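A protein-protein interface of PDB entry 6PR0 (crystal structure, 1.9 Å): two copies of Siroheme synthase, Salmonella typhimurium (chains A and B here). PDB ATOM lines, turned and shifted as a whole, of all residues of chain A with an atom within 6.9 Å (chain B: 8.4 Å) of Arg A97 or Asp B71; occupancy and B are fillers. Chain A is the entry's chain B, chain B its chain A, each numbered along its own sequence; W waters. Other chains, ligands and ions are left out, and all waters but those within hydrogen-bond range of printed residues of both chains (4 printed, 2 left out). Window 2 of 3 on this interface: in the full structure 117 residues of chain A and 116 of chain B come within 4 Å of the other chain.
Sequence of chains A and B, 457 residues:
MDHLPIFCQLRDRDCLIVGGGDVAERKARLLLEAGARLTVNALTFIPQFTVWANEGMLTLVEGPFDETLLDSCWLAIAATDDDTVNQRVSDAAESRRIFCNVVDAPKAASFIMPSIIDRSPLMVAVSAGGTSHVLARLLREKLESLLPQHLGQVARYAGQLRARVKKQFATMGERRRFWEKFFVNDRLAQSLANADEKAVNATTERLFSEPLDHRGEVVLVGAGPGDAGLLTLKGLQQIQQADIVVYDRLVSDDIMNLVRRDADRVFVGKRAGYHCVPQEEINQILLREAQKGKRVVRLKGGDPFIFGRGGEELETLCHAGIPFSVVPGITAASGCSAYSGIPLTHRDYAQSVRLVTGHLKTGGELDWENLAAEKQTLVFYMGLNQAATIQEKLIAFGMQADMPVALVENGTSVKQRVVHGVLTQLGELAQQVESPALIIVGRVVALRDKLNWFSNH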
ATOM      1  N   CYS A  73       4.982  -5.079 -21.965  1.00  0.00           N
ATOM      2  CA  CYS A  73       3.968  -5.396 -20.976  1.00  0.00           C
ATOM      3  C   CYS A  73       3.245  -6.696 -21.309  1.00  0.00           C
ATOM      4  O   CYS A  73       3.000  -6.998 -22.481  1.00  0.00           O
ATOM      5  CB  CYS A  73       2.957  -4.254 -20.915  1.00  0.00           C
ATOM      6  SG  CYS A  73       2.172  -4.080 -19.352  1.00  0.00           S
ATOM      7  N   TRP A  74       2.889  -7.449 -20.262  1.00  0.00           N
ATOM      8  CA  TRP A  74       2.015  -8.613 -20.370  1.00  0.00           C
ATOM      9  C   TRP A  74       0.594  -8.348 -19.881  1.00  0.00           C
ATOM     10  O   TRP A  74      -0.327  -9.059 -20.287  1.00  0.00           O
ATOM     11  CB  TRP A  74       2.573  -9.792 -19.546  1.00  0.00           C
ATOM     12  CG  TRP A  74       3.883 -10.388 -20.036  1.00  0.00           C
ATOM     13  CD1 TRP A  74       5.128  -9.797 -20.014  1.00  0.00           C
ATOM     14  CD2 TRP A  74       4.068 -11.676 -20.629  1.00  0.00           C
ATOM     15  NE1 TRP A  74       6.070 -10.649 -20.543  1.00  0.00           N
ATOM     16  CE2 TRP A  74       5.446 -11.806 -20.934  1.00  0.00           C
ATOM     17  CE3 TRP A  74       3.205 -12.742 -20.926  1.00  0.00           C
ATOM     18  CZ2 TRP A  74       5.978 -12.954 -21.521  1.00  0.00           C
ATOM     19  CZ3 TRP A  74       3.738 -13.883 -21.518  1.00  0.00           C
ATOM     20  CH2 TRP A  74       5.115 -13.980 -21.802  1.00  0.00           C
ATOM     21  N   ALA A  92      -4.487   1.746 -26.171  1.00  0.00           N
ATOM     22  CA  ALA A  92      -3.077   1.455 -26.395  1.00  0.00           C
ATOM     23  C   ALA A  92      -2.759  -0.003 -26.069  1.00  0.00           C
ATOM     24  O   ALA A  92      -1.968  -0.646 -26.776  1.00  0.00           O
ATOM     25  CB  ALA A  92      -2.208   2.403 -25.566  1.00  0.00           C
ATOM     26  N   ALA A  93      -3.381  -0.549 -25.022  1.00  0.00           N
ATOM     27  CA  ALA A  93      -3.199  -1.974 -24.739  1.00  0.00           C
ATOM     28  C   ALA A  93      -3.818  -2.848 -25.828  1.00  0.00           C
ATOM     29  O   ALA A  93      -3.251  -3.880 -26.211  1.00  0.00           O
ATOM     30  CB  ALA A  93      -3.802  -2.317 -23.377  1.00  0.00           C
ATOM     31  N   GLU A  94      -4.994  -2.474 -26.328  1.00  0.00           N
ATOM     32  CA  GLU A  94      -5.657  -3.302 -27.332  1.00  0.00           C
ATOM     33  C   GLU A  94      -4.848  -3.371 -28.619  1.00  0.00           C
ATOM     34  O   GLU A  94      -4.728  -4.438 -29.240  1.00  0.00           O
ATOM     35  CB  GLU A  94      -7.056  -2.758 -27.604  1.00  0.00           C
ATOM     36  CG  GLU A  94      -7.658  -3.206 -28.925  1.00  0.00           C
ATOM     37  CD  GLU A  94      -8.538  -4.418 -28.761  1.00  0.00           C
ATOM     38  OE1 GLU A  94      -9.035  -4.945 -29.775  1.00  0.00           O
ATOM     39  OE2 GLU A  94      -8.724  -4.854 -27.609  1.00  0.00           O
ATOM     40  N   SER A  95      -4.294  -2.242 -29.051  1.00  0.00           N
ATOM     41  CA  SER A  95      -3.504  -2.274 -30.276  1.00  0.00           C
ATOM     42  C   SER A  95      -2.253  -3.127 -30.112  1.00  0.00           C
ATOM     43  O   SER A  95      -1.705  -3.603 -31.110  1.00  0.00           O
ATOM     44  CB  SER A  95      -3.130  -0.853 -30.707  1.00  0.00           C
ATOM     45  OG  SER A  95      -2.149  -0.313 -29.837  1.00  0.00           O
ATOM     46  N   ARG A  96      -1.806  -3.362 -28.882  1.00  0.00           N
ATOM     47  CA  ARG A  96      -0.644  -4.207 -28.657  1.00  0.00           C
ATOM     48  C   ARG A  96      -1.008  -5.629 -28.237  1.00  0.00           C
ATOM     49  O   ARG A  96      -0.111  -6.396 -27.881  1.00  0.00           O
ATOM     50  CB  ARG A  96       0.254  -3.573 -27.607  1.00  0.00           C
ATOM     51  CG  ARG A  96       0.877  -2.276 -28.058  1.00  0.00           C
ATOM     52  CD  ARG A  96       1.564  -1.595 -26.886  1.00  0.00           C
ATOM     53  NE  ARG A  96       2.337  -0.421 -27.282  1.00  0.00           N
ATOM     54  CZ  ARG A  96       1.806   0.747 -27.617  1.00  0.00           C
ATOM     55  NH1 ARG A  96       0.489   0.901 -27.627  1.00  0.00           N
ATOM     56  NH2 ARG A  96       2.598   1.763 -27.962  1.00  0.00           N
ATOM     57  N   ARG A  97      -2.292  -5.980 -28.255  1.00  0.00           N
ATOM     58  CA  ARG A  97      -2.780  -7.291 -27.816  1.00  0.00           C
ATOM     59  C   ARG A  97      -2.320  -7.621 -26.394  1.00  0.00           C
ATOM     60  O   ARG A  97      -1.876  -8.729 -26.098  1.00  0.00           O
ATOM     61  CB  ARG A  97      -2.369  -8.387 -28.800  1.00  0.00           C
ATOM     62  CG  ARG A  97      -2.980  -8.190 -30.192  1.00  0.00           C
ATOM     63  CD  ARG A  97      -2.211  -8.933 -31.275  1.00  0.00           C
ATOM     64  NE  ARG A  97      -0.760  -8.763 -31.171  1.00  0.00           N
ATOM     65  CZ  ARG A  97      -0.052  -7.936 -31.933  1.00  0.00           C
ATOM     66  NH1 ARG A  97      -0.662  -7.195 -32.849  1.00  0.00           N
ATOM     67  NH2 ARG A  97       1.264  -7.842 -31.772  1.00  0.00           N
ATOM     68  N   ILE A  98      -2.452  -6.648 -25.500  1.00  0.00           N
ATOM     69  CA  ILE A  98      -2.129  -6.809 -24.085  1.00  0.00           C
ATOM     70  C   ILE A  98      -3.442  -6.847 -23.317  1.00  0.00           C
ATOM     71  O   ILE A  98      -4.215  -5.884 -23.366  1.00  0.00           O
ATOM     72  CB  ILE A  98      -1.260  -5.650 -23.569  1.00  0.00           C
ATOM     73  CG1 ILE A  98       0.129  -5.634 -24.213  1.00  0.00           C
ATOM     74  CG2 ILE A  98      -1.195  -5.665 -22.025  1.00  0.00           C
ATOM     75  CD1 ILE A  98       0.885  -4.281 -23.949  1.00  0.00           C
ATOM     76  N   PHE A  99      -3.696  -7.939 -22.598  1.00  0.00           N
ATOM     77  CA  PHE A  99      -4.922  -8.009 -21.810  1.00  0.00           C
ATOM     78  C   PHE A  99      -4.962  -6.867 -20.815  1.00  0.00           C
ATOM     79  O   PHE A  99      -3.970  -6.587 -20.135  1.00  0.00           O
ATOM     80  CB  PHE A  99      -5.026  -9.354 -21.092  1.00  0.00           C
ATOM     81  CG  PHE A  99      -5.503 -10.458 -21.988  1.00  0.00           C
ATOM     82  CD1 PHE A  99      -4.633 -11.435 -22.424  1.00  0.00           C
ATOM     83  CD2 PHE A  99      -6.816 -10.474 -22.443  1.00  0.00           C
ATOM     84  CE1 PHE A  99      -5.067 -12.456 -23.282  1.00  0.00           C
ATOM     85  CE2 PHE A  99      -7.261 -11.497 -23.281  1.00  0.00           C
ATOM     86  CZ  PHE A  99      -6.386 -12.476 -23.706  1.00  0.00           C
ATOM     87  N   SER A 110     -10.343  -6.019 -21.888  1.00  0.00           N
ATOM     88  CA  SER A 110     -10.211  -7.392 -22.346  1.00  0.00           C
ATOM     89  C   SER A 110     -10.127  -8.425 -21.226  1.00  0.00           C
ATOM     90  O   SER A 110     -10.146  -9.623 -21.520  1.00  0.00           O
ATOM     91  CB  SER A 110      -8.995  -7.506 -23.269  1.00  0.00           C
ATOM     92  OG  SER A 110      -7.929  -6.722 -22.763  1.00  0.00           O
ATOM     93  N   ARG B  13     -11.002 -12.430 -30.836  1.00  0.00           N
ATOM     94  CA  ARG B  13      -9.567 -12.254 -30.675  1.00  0.00           C
ATOM     95  C   ARG B  13      -8.843 -13.506 -31.166  1.00  0.00           C
ATOM     96  O   ARG B  13      -9.284 -14.627 -30.907  1.00  0.00           O
ATOM     97  CB  ARG B  13      -9.210 -11.953 -29.213  1.00  0.00           C
ATOM     98  CG  ARG B  13      -9.939 -10.709 -28.670  1.00  0.00           C
ATOM     99  CD  ARG B  13      -9.328 -10.125 -27.387  1.00  0.00           C
ATOM    100  NE  ARG B  13      -9.522  -8.673 -27.368  1.00  0.00           N
ATOM    101  CZ  ARG B  13     -10.483  -8.032 -26.702  1.00  0.00           C
ATOM    102  NH1 ARG B  13     -11.361  -8.688 -25.946  1.00  0.00           N
ATOM    103  NH2 ARG B  13     -10.565  -6.716 -26.792  1.00  0.00           N
ATOM    104  N   ASP B  14      -7.748 -13.318 -31.895  1.00  0.00           N
ATOM    105  CA  ASP B  14      -7.038 -14.457 -32.468  1.00  0.00           C
ATOM    106  C   ASP B  14      -6.350 -15.265 -31.376  1.00  0.00           C
ATOM    107  O   ASP B  14      -5.637 -14.704 -30.538  1.00  0.00           O
ATOM    108  CB  ASP B  14      -5.992 -13.993 -33.488  1.00  0.00           C
ATOM    109  CG  ASP B  14      -6.602 -13.222 -34.658  1.00  0.00           C
ATOM    110  OD1 ASP B  14      -7.820 -13.341 -34.885  1.00  0.00           O
ATOM    111  OD2 ASP B  14      -5.859 -12.497 -35.351  1.00  0.00           O
ATOM    112  N   LEU B  16      -4.217 -19.302 -30.952  1.00  0.00           N
ATOM    113  CA  LEU B  16      -3.593 -20.387 -31.695  1.00  0.00           C
ATOM    114  C   LEU B  16      -3.480 -21.640 -30.843  1.00  0.00           C
ATOM    115  O   LEU B  16      -3.035 -21.574 -29.690  1.00  0.00           O
ATOM    116  CB  LEU B  16      -2.195 -19.978 -32.187  1.00  0.00           C
ATOM    117  CG  LEU B  16      -1.418 -21.080 -32.934  1.00  0.00           C
ATOM    118  CD1 LEU B  16      -2.028 -21.331 -34.315  1.00  0.00           C
ATOM    119  CD2 LEU B  16       0.043 -20.725 -33.079  1.00  0.00           C
ATOM    120  N   ASP B  66       4.266 -23.179 -37.358  1.00  0.00           N
ATOM    121  CA  ASP B  66       4.623 -21.943 -38.054  1.00  0.00           C
ATOM    122  C   ASP B  66       4.513 -20.824 -37.031  1.00  0.00           C
ATOM    123  O   ASP B  66       3.402 -20.418 -36.676  1.00  0.00           O
ATOM    124  CB  ASP B  66       3.694 -21.708 -39.252  1.00  0.00           C
ATOM    125  CG  ASP B  66       3.932 -20.363 -39.954  1.00  0.00           C
ATOM    126  OD1 ASP B  66       4.848 -19.611 -39.566  1.00  0.00           O
ATOM    127  OD2 ASP B  66       3.202 -20.066 -40.930  1.00  0.00           O
ATOM    128  N   GLU B  67       5.650 -20.328 -36.543  1.00  0.00           N
ATOM    129  CA  GLU B  67       5.584 -19.341 -35.472  1.00  0.00           C
ATOM    130  C   GLU B  67       5.021 -17.997 -35.945  1.00  0.00           C
ATOM    131  O   GLU B  67       4.567 -17.205 -35.112  1.00  0.00           O
ATOM    132  CB  GLU B  67       6.963 -19.128 -34.849  1.00  0.00           C
ATOM    133  CG  GLU B  67       7.952 -18.425 -35.748  1.00  0.00           C
ATOM    134  CD  GLU B  67       9.298 -18.239 -35.056  1.00  0.00           C
ATOM    135  OE1 GLU B  67       9.307 -17.915 -33.843  1.00  0.00           O
ATOM    136  OE2 GLU B  67      10.344 -18.439 -35.715  1.00  0.00           O
ATOM    137  N   THR B  68       5.042 -17.713 -37.241  1.00  0.00           N
ATOM    138  CA  THR B  68       4.395 -16.477 -37.674  1.00  0.00           C
ATOM    139  C   THR B  68       2.895 -16.498 -37.407  1.00  0.00           C
ATOM    140  O   THR B  68       2.275 -15.427 -37.381  1.00  0.00           O
ATOM    141  CB  THR B  68       4.652 -16.203 -39.151  1.00  0.00           C
ATOM    142  OG1 THR B  68       3.912 -17.116 -39.961  1.00  0.00           O
ATOM    143  CG2 THR B  68       6.130 -16.321 -39.468  1.00  0.00           C
ATOM    144  N   LEU B  69       2.300 -17.689 -37.214  1.00  0.00           N
ATOM    145  CA  LEU B  69       0.885 -17.776 -36.843  1.00  0.00           C
ATOM    146  C   LEU B  69       0.601 -17.150 -35.485  1.00  0.00           C
ATOM    147  O   LEU B  69      -0.567 -16.886 -35.162  1.00  0.00           O
ATOM    148  CB  LEU B  69       0.418 -19.235 -36.830  1.00  0.00           C
ATOM    149  CG  LEU B  69       0.226 -19.904 -38.199  1.00  0.00           C
ATOM    150  CD1 LEU B  69      -0.208 -21.342 -38.045  1.00  0.00           C
ATOM    151  CD2 LEU B  69      -0.771 -19.126 -39.050  1.00  0.00           C
ATOM    152  N   LEU B  70       1.634 -16.918 -34.673  1.00  0.00           N
ATOM    153  CA  LEU B  70       1.452 -16.217 -33.406  1.00  0.00           C
ATOM    154  C   LEU B  70       1.345 -14.703 -33.555  1.00  0.00           C
ATOM    155  O   LEU B  70       1.016 -14.029 -32.574  1.00  0.00           O
ATOM    156  CB  LEU B  70       2.616 -16.514 -32.471  1.00  0.00           C
ATOM    157  CG  LEU B  70       2.628 -17.960 -31.935  1.00  0.00           C
ATOM    158  CD1 LEU B  70       3.960 -18.229 -31.268  1.00  0.00           C
ATOM    159  CD2 LEU B  70       1.483 -18.189 -30.957  1.00  0.00           C
ATOM    160  N   ASP B  71       1.626 -14.147 -34.736  1.00  0.00           N
ATOM    161  CA  ASP B  71       1.888 -12.710 -34.818  1.00  0.00           C
ATOM    162  C   ASP B  71       0.700 -11.862 -34.381  1.00  0.00           C
ATOM    163  O   ASP B  71       0.890 -10.763 -33.846  1.00  0.00           O
ATOM    164  CB  ASP B  71       2.315 -12.330 -36.234  1.00  0.00           C
ATOM    165  CG  ASP B  71       3.721 -12.815 -36.558  1.00  0.00           C
ATOM    166  OD1 ASP B  71       4.377 -13.366 -35.653  1.00  0.00           O
ATOM    167  OD2 ASP B  71       4.166 -12.660 -37.708  1.00  0.00           O
ATOM    168  N   SER B  72      -0.525 -12.336 -34.581  1.00  0.00           N
ATOM    169  CA  SER B  72      -1.691 -11.536 -34.213  1.00  0.00           C
ATOM    170  C   SER B  72      -2.436 -12.107 -33.007  1.00  0.00           C
ATOM    171  O   SER B  72      -3.588 -11.734 -32.761  1.00  0.00           O
ATOM    172  CB  SER B  72      -2.639 -11.404 -35.407  1.00  0.00           C
ATOM    173  OG  SER B  72      -3.097 -12.681 -35.844  1.00  0.00           O
ATOM    174  N   CYS B  73      -1.805 -12.995 -32.244  1.00  0.00           N
ATOM    175  CA  CYS B  73      -2.517 -13.812 -31.271  1.00  0.00           C
ATOM    176  C   CYS B  73      -2.480 -13.215 -29.865  1.00  0.00           C
ATOM    177  O   CYS B  73      -1.523 -12.540 -29.464  1.00  0.00           O
ATOM    178  CB  CYS B  73      -1.946 -15.237 -31.233  1.00  0.00           C
ATOM    179  SG  CYS B  73      -2.569 -16.242 -32.611  1.00  0.00           S
ATOM    180  N   TRP B  74      -3.531 -13.525 -29.104  1.00  0.00           N
ATOM    181  CA  TRP B  74      -3.651 -13.119 -27.719  1.00  0.00           C
ATOM    182  C   TRP B  74      -3.386 -14.261 -26.749  1.00  0.00           C
ATOM    183  O   TRP B  74      -3.059 -14.004 -25.587  1.00  0.00           O
ATOM    184  CB  TRP B  74      -5.050 -12.562 -27.454  1.00  0.00           C
ATOM    185  CG  TRP B  74      -5.437 -11.276 -28.162  1.00  0.00           C
ATOM    186  CD1 TRP B  74      -5.690 -11.089 -29.506  1.00  0.00           C
ATOM    187  CD2 TRP B  74      -5.703 -10.031 -27.529  1.00  0.00           C
ATOM    188  NE1 TRP B  74      -6.087  -9.784 -29.741  1.00  0.00           N
ATOM    189  CE2 TRP B  74      -6.090  -9.112 -28.541  1.00  0.00           C
ATOM    190  CE3 TRP B  74      -5.637  -9.591 -26.200  1.00  0.00           C
ATOM    191  CZ2 TRP B  74      -6.410  -7.787 -28.259  1.00  0.00           C
ATOM    192  CZ3 TRP B  74      -5.952  -8.259 -25.919  1.00  0.00           C
ATOM    193  CH2 TRP B  74      -6.338  -7.374 -26.952  1.00  0.00           C
ATOM    194  N   LEU B  75      -3.526 -15.508 -27.197  1.00  0.00           N
ATOM    195  CA  LEU B  75      -3.331 -16.681 -26.365  1.00  0.00           C
ATOM    196  C   LEU B  75      -2.836 -17.787 -27.272  1.00  0.00           C
ATOM    197  O   LEU B  75      -3.276 -17.898 -28.421  1.00  0.00           O
ATOM    198  CB  LEU B  75      -4.625 -17.159 -25.675  1.00  0.00           C
ATOM    199  CG  LEU B  75      -5.252 -16.426 -24.506  1.00  0.00           C
ATOM    200  CD1 LEU B  75      -6.492 -17.212 -24.073  1.00  0.00           C
ATOM    201  CD2 LEU B  75      -4.257 -16.323 -23.344  1.00  0.00           C
ATOM    202  N   ALA B  92       8.385 -19.187 -28.668  1.00  0.00           N
ATOM    203  CA  ALA B  92       7.933 -18.191 -29.630  1.00  0.00           C
ATOM    204  C   ALA B  92       6.863 -17.291 -29.022  1.00  0.00           C
ATOM    205  O   ALA B  92       6.860 -16.074 -29.262  1.00  0.00           O
ATOM    206  CB  ALA B  92       7.410 -18.889 -30.882  1.00  0.00           C
ATOM    207  N   SER B  95       8.508 -14.766 -26.498  1.00  0.00           N
ATOM    208  CA  SER B  95       9.177 -13.636 -27.137  1.00  0.00           C
ATOM    209  C   SER B  95       8.178 -12.575 -27.571  1.00  0.00           C
ATOM    210  O   SER B  95       8.525 -11.392 -27.640  1.00  0.00           O
ATOM    211  CB  SER B  95      10.011 -14.098 -28.334  1.00  0.00           C
ATOM    212  OG  SER B  95       9.198 -14.453 -29.440  1.00  0.00           O
ATOM    213  N   ARG B  96       6.935 -12.969 -27.835  1.00  0.00           N
ATOM    214  CA  ARG B  96       5.881 -12.040 -28.247  1.00  0.00           C
ATOM    215  C   ARG B  96       5.000 -11.577 -27.080  1.00  0.00           C
ATOM    216  O   ARG B  96       4.021 -10.857 -27.303  1.00  0.00           O
ATOM    217  CB  ARG B  96       5.010 -12.681 -29.339  1.00  0.00           C
ATOM    218  CG  ARG B  96       5.796 -13.051 -30.618  1.00  0.00           C
ATOM    219  CD  ARG B  96       4.985 -13.905 -31.576  1.00  0.00           C
ATOM    220  NE  ARG B  96       5.580 -13.985 -32.916  1.00  0.00           N
ATOM    221  CZ  ARG B  96       6.639 -14.731 -33.231  1.00  0.00           C
ATOM    222  NH1 ARG B  96       7.236 -15.470 -32.310  1.00  0.00           N
ATOM    223  NH2 ARG B  96       7.103 -14.752 -34.473  1.00  0.00           N
ATOM    224  N   ARG B  97       5.340 -11.962 -25.849  1.00  0.00           N
ATOM    225  CA  ARG B  97       4.544 -11.670 -24.656  1.00  0.00           C
ATOM    226  C   ARG B  97       3.100 -12.144 -24.834  1.00  0.00           C
ATOM    227  O   ARG B  97       2.130 -11.442 -24.531  1.00  0.00           O
ATOM    228  CB  ARG B  97       4.614 -10.181 -24.301  1.00  0.00           C
ATOM    229  CG  ARG B  97       6.049  -9.720 -23.998  1.00  0.00           C
ATOM    230  CD  ARG B  97       6.143  -8.222 -23.999  1.00  0.00           C
ATOM    231  NE  ARG B  97       5.742  -7.678 -25.292  1.00  0.00           N
ATOM    232  CZ  ARG B  97       6.552  -7.597 -26.341  1.00  0.00           C
ATOM    233  NH1 ARG B  97       7.813  -8.007 -26.242  1.00  0.00           N
ATOM    234  NH2 ARG B  97       6.107  -7.094 -27.483  1.00  0.00           N
ATOM    235  N   ILE B  98       2.961 -13.351 -25.358  1.00  0.00           N
ATOM    236  CA  ILE B  98       1.660 -13.984 -25.518  1.00  0.00           C
ATOM    237  C   ILE B  98       1.524 -15.024 -24.424  1.00  0.00           C
ATOM    238  O   ILE B  98       2.342 -15.941 -24.341  1.00  0.00           O
ATOM    239  CB  ILE B  98       1.512 -14.627 -26.903  1.00  0.00           C
ATOM    240  CG1 ILE B  98       1.578 -13.545 -27.993  1.00  0.00           C
ATOM    241  CG2 ILE B  98       0.174 -15.446 -26.956  1.00  0.00           C
ATOM    242  CD1 ILE B  98       1.733 -14.150 -29.420  1.00  0.00           C
ATOM    243  N   PHE B  99       0.487 -14.905 -23.595  1.00  0.00           N
ATOM    244  CA  PHE B  99       0.248 -15.947 -22.611  1.00  0.00           C
ATOM    245  C   PHE B  99       0.063 -17.299 -23.297  1.00  0.00           C
ATOM    246  O   PHE B  99      -0.678 -17.418 -24.277  1.00  0.00           O
ATOM    247  CB  PHE B  99      -0.962 -15.579 -21.744  1.00  0.00           C
ATOM    248  CG  PHE B  99      -0.610 -14.636 -20.628  1.00  0.00           C
ATOM    249  CD1 PHE B  99       0.200 -15.063 -19.587  1.00  0.00           C
ATOM    250  CD2 PHE B  99      -1.034 -13.312 -20.651  1.00  0.00           C
ATOM    251  CE1 PHE B  99       0.564 -14.190 -18.561  1.00  0.00           C
ATOM    252  CE2 PHE B  99      -0.695 -12.436 -19.634  1.00  0.00           C
ATOM    253  CZ  PHE B  99       0.128 -12.873 -18.589  1.00  0.00           C
HETATM  254  O   HOH W   1       0.012  -8.641 -35.489  1.00  0.00           O
HETATM  255  O   HOH W   2       3.270  -6.589 -25.236  1.00  0.00           O
HETATM  256  O   HOH W   3       0.842 -10.772 -29.998  1.00  0.00           O
HETATM  257  O   HOH W   4       1.098  -8.954 -24.101  1.00  0.00           O
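Water W2 lies within hydrogen-bond range of NE of Arg B97 (2.7 Å) and O of Cys A73 (2.8 Å).
Water W4 lies within hydrogen-bond range of O of Arg B97 and O of Cys A73.
Water W1 lies within hydrogen-bond range of O of Asp B71 (2.8 Å) and NH1 of Arg A97 (3.1 Å).
Water W3 bridges NE of Arg A97 (2.8 Å) and O of Cys B73 (3.0 Å).
Hydrophobic or aromatic side chains of chain A within 4 Å of the printed part of chain B: Trp A74 and Phe A99.
Of the 19 printed residues of chain B, 8 touch a printed residue of chain A.
Hydrophobic or aromatic side chains of chain B within 4 Å of the printed part of chain A: Trp B74, Leu B75 and Phe B99.
Among the printed residues, Asp or Glu carboxylates within 4 Å of a Lys or Arg side-chain nitrogen of the other chain: Glu A94 with Arg B13 (2.7 Å).
OG of Ser B72 is in hydrogen-bond range of OD2 of Asp B14 (2.8 Å).
N of Trp B74 lies within hydrogen-bond range of O of Asp B14 (2.8 Å).
The backbone carbonyl oxygen (O) of Leu B75 is in hydrogen-bond range of the backbone NH (N) of Leu B16 (3.0 Å).
The side-chain carboxylate (OD1) of Asp B71 lies within salt-bridge range of the guanidinium group (NE) of Arg B96.
O of Ala A93 is in hydrogen-bond range of N of Ile A98 (3.0 Å).
Arg A97 touches just these residues of chain B: Asp B71, Ser B72 and Trp B74.
Printed residues of chain A within 4 Å of Arg B13: Glu A94 and Ser A110.
Thr B68 touches none of the printed residues of chain A.
Asp B71 touches just one residue of chain A: Arg A97 (3.5 Å).
Printed residues of chain A within 4 Å of Ser B72: Arg A97 (3.5 Å).
Of the printed residues of chain A, Arg B97 touches Cys A73 and Trp A74.
The nearest residue of chain B that does not touch Arg A97 is Cys B73 (4.1 Å).
The nearest printed residue of chain B that does not touch Glu A94 is Ser B72 (8.2 Å).
Among the printed residues, merely in contact across the chains: Cys A73 with Arg B97 (3.7 Å), Trp A74 with Arg B97 (3.6 Å), Trp A74 with Ile B98 (3.8 Å), Trp A74 with Phe B99 (3.5 Å), Glu A94 with Trp B74 (3.5 Å), Arg A97 with Asp B71 (3.5 Å), Arg A97 with Ser B72 (3.5 Å), Arg A97 with Trp B74 (3.5 Å), Ile A98 with Trp B74 (3.9 Å), Phe A99 with Trp B74 (3.4 Å), Phe A99 with Leu B75 (3.95 Å) and Ser A110 with Arg B13 (3.8 Å).
Cys A73 touches Arg B97, but with the chains exchanged Arg A97 does not touch Cys B73 (4.1 Å).
Trp A74 touches Arg B97, and with the chains exchanged Arg A97 touches Trp B74.
Trp A74 touches Ile B98, and with the chains exchanged Ile A98 touches Trp B74.
Trp A74 touches Phe B99, and with the chains exchanged Phe A99 touches Trp B74.
Positions printed for both chains: 73, 74, 92, 95, 96, 97, 98 and 99.
Of the 13 pairs that touch across the chains among the printed residues, 6 have their exchanged pair printed and touching as well.
The guanidinium group (NH2) of Arg B13 lies within salt-bridge range of the side-chain carboxylate (OE2) of Glu A94 (2.7 Å).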
